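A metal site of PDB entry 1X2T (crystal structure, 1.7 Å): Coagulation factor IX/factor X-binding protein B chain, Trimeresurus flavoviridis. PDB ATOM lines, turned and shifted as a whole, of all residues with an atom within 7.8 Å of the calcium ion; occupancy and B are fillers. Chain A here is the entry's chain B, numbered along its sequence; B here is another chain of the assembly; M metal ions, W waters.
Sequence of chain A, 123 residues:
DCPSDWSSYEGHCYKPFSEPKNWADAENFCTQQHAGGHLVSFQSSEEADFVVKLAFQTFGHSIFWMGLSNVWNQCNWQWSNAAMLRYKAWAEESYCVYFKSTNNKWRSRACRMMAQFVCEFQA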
ATOM      1  N   TYR A   9      12.359   0.397  31.683  1.00  0.00           N
ATOM      2  CA  TYR A   9      13.214  -0.658  31.154  1.00  0.00           C
ATOM      3  C   TYR A   9      13.824  -0.150  29.845  1.00  0.00           C
ATOM      4  O   TYR A   9      13.106   0.101  28.876  1.00  0.00           O
ATOM      5  CB  TYR A   9      12.446  -1.953  30.877  1.00  0.00           C
ATOM      6  CG  TYR A   9      13.311  -3.001  30.205  1.00  0.00           C
ATOM      7  CD1 TYR A   9      14.258  -3.721  30.928  1.00  0.00           C
ATOM      8  CD2 TYR A   9      13.228  -3.213  28.827  1.00  0.00           C
ATOM      9  CE1 TYR A   9      15.109  -4.647  30.288  1.00  0.00           C
ATOM     10  CE2 TYR A   9      14.067  -4.119  28.184  1.00  0.00           C
ATOM     11  CZ  TYR A   9      15.006  -4.826  28.924  1.00  0.00           C
ATOM     12  OH  TYR A   9      15.833  -5.721  28.268  1.00  0.00           O
ATOM     13  N   HIS A  12      12.175   2.718  27.969  1.00  0.00           N
ATOM     14  CA  HIS A  12      10.742   2.624  27.743  1.00  0.00           C
ATOM     15  C   HIS A  12      10.021   2.544  29.072  1.00  0.00           C
ATOM     16  O   HIS A  12      10.622   2.229  30.107  1.00  0.00           O
ATOM     17  CB  HIS A  12      10.383   1.397  26.904  1.00  0.00           C
ATOM     18  CG  HIS A  12      10.740   1.521  25.446  1.00  0.00           C
ATOM     19  ND1 HIS A  12      10.061   0.846  24.460  1.00  0.00           N
ATOM     20  CD2 HIS A  12      11.711   2.231  24.820  1.00  0.00           C
ATOM     21  CE1 HIS A  12      10.597   1.136  23.288  1.00  0.00           C
ATOM     22  NE2 HIS A  12      11.598   1.979  23.483  1.00  0.00           N
ATOM     23  N   TYR A  14       6.543   0.993  31.113  1.00  0.00           N
ATOM     24  CA  TYR A  14       5.516  -0.031  31.073  1.00  0.00           C
ATOM     25  C   TYR A  14       4.593   0.062  32.267  1.00  0.00           C
ATOM     26  O   TYR A  14       4.999   0.495  33.358  1.00  0.00           O
ATOM     27  CB  TYR A  14       6.160  -1.423  31.059  1.00  0.00           C
ATOM     28  CG  TYR A  14       7.239  -1.604  30.015  1.00  0.00           C
ATOM     29  CD1 TYR A  14       8.501  -1.037  30.181  1.00  0.00           C
ATOM     30  CD2 TYR A  14       6.981  -2.343  28.861  1.00  0.00           C
ATOM     31  CE1 TYR A  14       9.491  -1.209  29.221  1.00  0.00           C
ATOM     32  CE2 TYR A  14       7.962  -2.518  27.892  1.00  0.00           C
ATOM     33  CZ  TYR A  14       9.216  -1.939  28.074  1.00  0.00           C
ATOM     34  OH  TYR A  14      10.195  -2.116  27.119  1.00  0.00           O
ATOM     35  N   LEU A  39      -0.253  -1.186  23.343  1.00  0.00           N
ATOM     36  CA  LEU A  39      -0.161  -2.427  24.095  1.00  0.00           C
ATOM     37  C   LEU A  39       1.312  -2.795  24.043  1.00  0.00           C
ATOM     38  O   LEU A  39       2.002  -2.439  23.084  1.00  0.00           O
ATOM     39  CB  LEU A  39      -0.999  -3.521  23.437  1.00  0.00           C
ATOM     40  CG  LEU A  39      -2.482  -3.534  23.826  1.00  0.00           C
ATOM     41  CD1 LEU A  39      -3.224  -4.577  23.017  1.00  0.00           C
ATOM     42  CD2 LEU A  39      -2.594  -3.830  25.306  1.00  0.00           C
ATOM     43  N   VAL A  40       1.813  -3.501  25.053  1.00  0.00           N
ATOM     44  CA  VAL A  40       3.226  -3.855  25.094  1.00  0.00           C
ATOM     45  C   VAL A  40       3.685  -4.727  23.928  1.00  0.00           C
ATOM     46  O   VAL A  40       2.960  -5.617  23.472  1.00  0.00           O
ATOM     47  CB  VAL A  40       3.605  -4.555  26.431  1.00  0.00           C
ATOM     48  CG1 VAL A  40       2.933  -5.914  26.545  1.00  0.00           C
ATOM     49  CG2 VAL A  40       5.111  -4.684  26.542  1.00  0.00           C
ATOM     50  N   SER A  41       4.890  -4.451  23.432  1.00  0.00           N
ATOM     51  CA  SER A  41       5.480  -5.180  22.326  1.00  0.00           C
ATOM     52  C   SER A  41       6.805  -5.782  22.801  1.00  0.00           C
ATOM     53  O   SER A  41       7.602  -5.092  23.436  1.00  0.00           O
ATOM     54  CB  SER A  41       5.745  -4.246  21.146  1.00  0.00           C
ATOM     55  OG  SER A  41       6.603  -3.184  21.545  1.00  0.00           O
ATOM     56  N   PHE A  42       7.022  -7.053  22.512  1.00  0.00           N
ATOM     57  CA  PHE A  42       8.262  -7.718  22.917  1.00  0.00           C
ATOM     58  C   PHE A  42       9.241  -7.819  21.761  1.00  0.00           C
ATOM     59  O   PHE A  42       9.027  -8.596  20.833  1.00  0.00           O
ATOM     60  CB  PHE A  42       7.989  -9.124  23.466  1.00  0.00           C
ATOM     61  CG  PHE A  42       7.193  -9.146  24.752  1.00  0.00           C
ATOM     62  CD1 PHE A  42       7.186  -8.044  25.606  1.00  0.00           C
ATOM     63  CD2 PHE A  42       6.468 -10.280  25.106  1.00  0.00           C
ATOM     64  CE1 PHE A  42       6.462  -8.073  26.793  1.00  0.00           C
ATOM     65  CE2 PHE A  42       5.749 -10.314  26.300  1.00  0.00           C
ATOM     66  CZ  PHE A  42       5.736  -9.206  27.148  1.00  0.00           C
ATOM     67  N   GLN A  43      10.307  -7.031  21.824  1.00  0.00           N
ATOM     68  CA  GLN A  43      11.336  -7.049  20.784  1.00  0.00           C
ATOM     69  C   GLN A  43      12.524  -7.910  21.187  1.00  0.00           C
ATOM     70  O   GLN A  43      13.439  -8.116  20.403  1.00  0.00           O
ATOM     71  CB  GLN A  43      11.822  -5.622  20.485  1.00  0.00           C
ATOM     72  CG  GLN A  43      10.979  -4.836  19.478  1.00  0.00           C
ATOM     73  CD  GLN A  43       9.664  -4.335  20.040  1.00  0.00           C
ATOM     74  OE1 GLN A  43       9.518  -4.154  21.251  1.00  0.00           O
ATOM     75  NE2 GLN A  43       8.702  -4.085  19.156  1.00  0.00           N
ATOM     76  N   SER A  44      12.500  -8.427  22.415  1.00  0.00           N
ATOM     77  CA  SER A  44      13.568  -9.277  22.929  1.00  0.00           C
ATOM     78  C   SER A  44      13.078 -10.105  24.111  1.00  0.00           C
ATOM     79  O   SER A  44      12.080  -9.773  24.743  1.00  0.00           O
ATOM     80  CB  SER A  44      14.773  -8.440  23.359  1.00  0.00           C
ATOM     81  OG  SER A  44      14.449  -7.614  24.467  1.00  0.00           O
ATOM     82  N   GLU A  47      13.297  -8.053  27.409  1.00  0.00           N
ATOM     83  CA  GLU A  47      12.215  -7.104  27.633  1.00  0.00           C
ATOM     84  C   GLU A  47      10.992  -7.881  28.098  1.00  0.00           C
ATOM     85  O   GLU A  47      10.264  -7.434  28.990  1.00  0.00           O
ATOM     86  CB  GLU A  47      11.909  -6.332  26.353  1.00  0.00           C
ATOM     87  CG  GLU A  47      10.618  -5.521  26.447  1.00  0.00           C
ATOM     88  CD  GLU A  47      10.244  -4.845  25.148  1.00  0.00           C
ATOM     89  OE1 GLU A  47      10.608  -5.378  24.071  1.00  0.00           O
ATOM     90  OE2 GLU A  47       9.587  -3.792  25.197  1.00  0.00           O
ATOM     91  N   ALA A  48      10.762  -9.034  27.501  1.00  0.00           N
ATOM     92  CA  ALA A  48       9.625  -9.866  27.880  1.00  0.00           C
ATOM     93  C   ALA A  48       9.760 -10.298  29.332  1.00  0.00           C
ATOM     94  O   ALA A  48       8.781 -10.275  30.087  1.00  0.00           O
ATOM     95  CB  ALA A  48       9.526 -11.094  26.971  1.00  0.00           C
ATOM     96  N   VAL A  51       8.756  -7.426  31.716  1.00  0.00           N
ATOM     97  CA  VAL A  51       7.307  -7.219  31.728  1.00  0.00           C
ATOM     98  C   VAL A  51       6.551  -8.357  32.412  1.00  0.00           C
ATOM     99  O   VAL A  51       5.591  -8.110  33.145  1.00  0.00           O
ATOM    100  CB  VAL A  51       6.773  -7.048  30.289  1.00  0.00           C
ATOM    101  CG1 VAL A  51       5.256  -6.895  30.299  1.00  0.00           C
ATOM    102  CG2 VAL A  51       7.422  -5.817  29.646  1.00  0.00           C
ATOM    103  N   GLU A 120       2.713   0.278  26.919  1.00  0.00           N
ATOM    104  CA  GLU A 120       4.107   0.676  26.759  1.00  0.00           C
ATOM    105  C   GLU A 120       4.273   1.916  25.893  1.00  0.00           C
ATOM    106  O   GLU A 120       3.494   2.158  24.968  1.00  0.00           O
ATOM    107  CB  GLU A 120       4.911  -0.479  26.133  1.00  0.00           C
ATOM    108  CG  GLU A 120       6.300  -0.078  25.640  1.00  0.00           C
ATOM    109  CD  GLU A 120       7.044  -1.215  24.956  1.00  0.00           C
ATOM    110  OE1 GLU A 120       6.384  -2.144  24.445  1.00  0.00           O
ATOM    111  OE2 GLU A 120       8.285  -1.176  24.919  1.00  0.00           O
ATOM    112  N   PHE A 121       5.299   2.706  26.193  1.00  0.00           N
ATOM    113  CA  PHE A 121       5.608   3.886  25.402  1.00  0.00           C
ATOM    114  C   PHE A 121       7.088   4.186  25.553  1.00  0.00           C
ATOM    115  O   PHE A 121       7.706   3.821  26.549  1.00  0.00           O
ATOM    116  CB  PHE A 121       4.731   5.083  25.801  1.00  0.00           C
ATOM    117  CG  PHE A 121       5.121   5.752  27.094  1.00  0.00           C
ATOM    118  CD1 PHE A 121       6.230   6.610  27.160  1.00  0.00           C
ATOM    119  CD2 PHE A 121       4.367   5.569  28.246  1.00  0.00           C
ATOM    120  CE1 PHE A 121       6.570   7.265  28.345  1.00  0.00           C
ATOM    121  CE2 PHE A 121       4.696   6.218  29.436  1.00  0.00           C
ATOM    122  CZ  PHE A 121       5.800   7.070  29.487  1.00  0.00           C
ATOM    123  N   TRP B  83       3.599  -4.812  15.018  1.00  0.00           N
ATOM    124  CA  TRP B  83       3.030  -4.590  16.349  1.00  0.00           C
ATOM    125  C   TRP B  83       2.144  -3.351  16.235  1.00  0.00           C
ATOM    126  O   TRP B  83       2.188  -2.661  15.220  1.00  0.00           O
ATOM    127  CB  TRP B  83       4.133  -4.313  17.377  1.00  0.00           C
ATOM    128  CG  TRP B  83       5.026  -5.479  17.667  1.00  0.00           C
ATOM    129  CD1 TRP B  83       6.217  -5.772  17.070  1.00  0.00           C
ATOM    130  CD2 TRP B  83       4.794  -6.501  18.642  1.00  0.00           C
ATOM    131  NE1 TRP B  83       6.742  -6.918  17.616  1.00  0.00           N
ATOM    132  CE2 TRP B  83       5.888  -7.379  18.586  1.00  0.00           C
ATOM    133  CE3 TRP B  83       3.765  -6.754  19.559  1.00  0.00           C
ATOM    134  CZ2 TRP B  83       5.992  -8.513  19.413  1.00  0.00           C
ATOM    135  CZ3 TRP B  83       3.861  -7.872  20.389  1.00  0.00           C
ATOM    136  CH2 TRP B  83       4.969  -8.739  20.300  1.00  0.00           C
ATOM    137  N   ASP B  85       2.538  -0.686  17.741  1.00  0.00           N
ATOM    138  CA  ASP B  85       3.391   0.497  17.826  1.00  0.00           C
ATOM    139  C   ASP B  85       4.015   0.803  16.467  1.00  0.00           C
ATOM    140  O   ASP B  85       4.738   1.787  16.320  1.00  0.00           O
ATOM    141  CB  ASP B  85       4.487   0.326  18.873  1.00  0.00           C
ATOM    142  CG  ASP B  85       5.441  -0.807  18.550  1.00  0.00           C
ATOM    143  OD1 ASP B  85       5.672  -1.083  17.360  1.00  0.00           O
ATOM    144  OD2 ASP B  85       5.983  -1.427  19.502  1.00  0.00           O
ATOM    145  N   SER B  87       6.234  -1.132  14.754  1.00  0.00           N
ATOM    146  CA  SER B  87       7.438  -1.918  14.493  1.00  0.00           C
ATOM    147  C   SER B  87       7.138  -3.280  13.897  1.00  0.00           C
ATOM    148  O   SER B  87       6.031  -3.804  14.033  1.00  0.00           O
ATOM    149  CB  SER B  87       8.238  -2.099  15.787  1.00  0.00           C
ATOM    150  OG  SER B  87       7.504  -2.826  16.751  1.00  0.00           O
HETATM  151 CA    CA M   1       8.591  -3.003  23.138  1.00  0.00          CA
HETATM  152  O   HOH W   1       8.410  -0.917  21.424  1.00  0.00           O
HETATM  153  O   HOH W   2      10.816  -2.218  23.063  1.00  0.00           O
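OE2 of Glu 120 lies close to ND1 of His 12 (2.7 Å). The side-chain carboxylate of Glu 120 sits close to the side-chain hydroxyl of Tyr 14 (3.1 Å). The side-chain hydroxyl of Ser 41 sits close to the side-chain carboxylate of Asp 85 of chain B, at 2.8 Å. The backbone NH of Glu 47 is in hydrogen-bond range of the side-chain hydroxyl of Ser 44 (3.2 Å). The side-chain amide nitrogen (NE2) of Gln 43 sits at hydrogen-bond distance from the side-chain hydroxyl (OG) of Ser 87 of chain B (3.0 Å). OE2 of Glu 47 sits close to OH of Tyr 14 (2.6 Å).
The nearest printed residue that does not touch the calcium ion is His 12 (4.3 Å).
The calcium ion is bound by the backbone carbonyl oxygen (O) of Ser 41, water W2, the side-chain amide oxygen (OE1) of Gln 43, the side-chain carboxylate (OE2) of Glu 47, the side-chain hydroxyl (OG) of Ser 41, the side-chain carboxylate (OE2) of Glu 120, the side-chain carboxylate (OE1) of Glu 120 and water W1.
Water W2 bridges OE1 of Glu 47 and ND1 of His 12.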
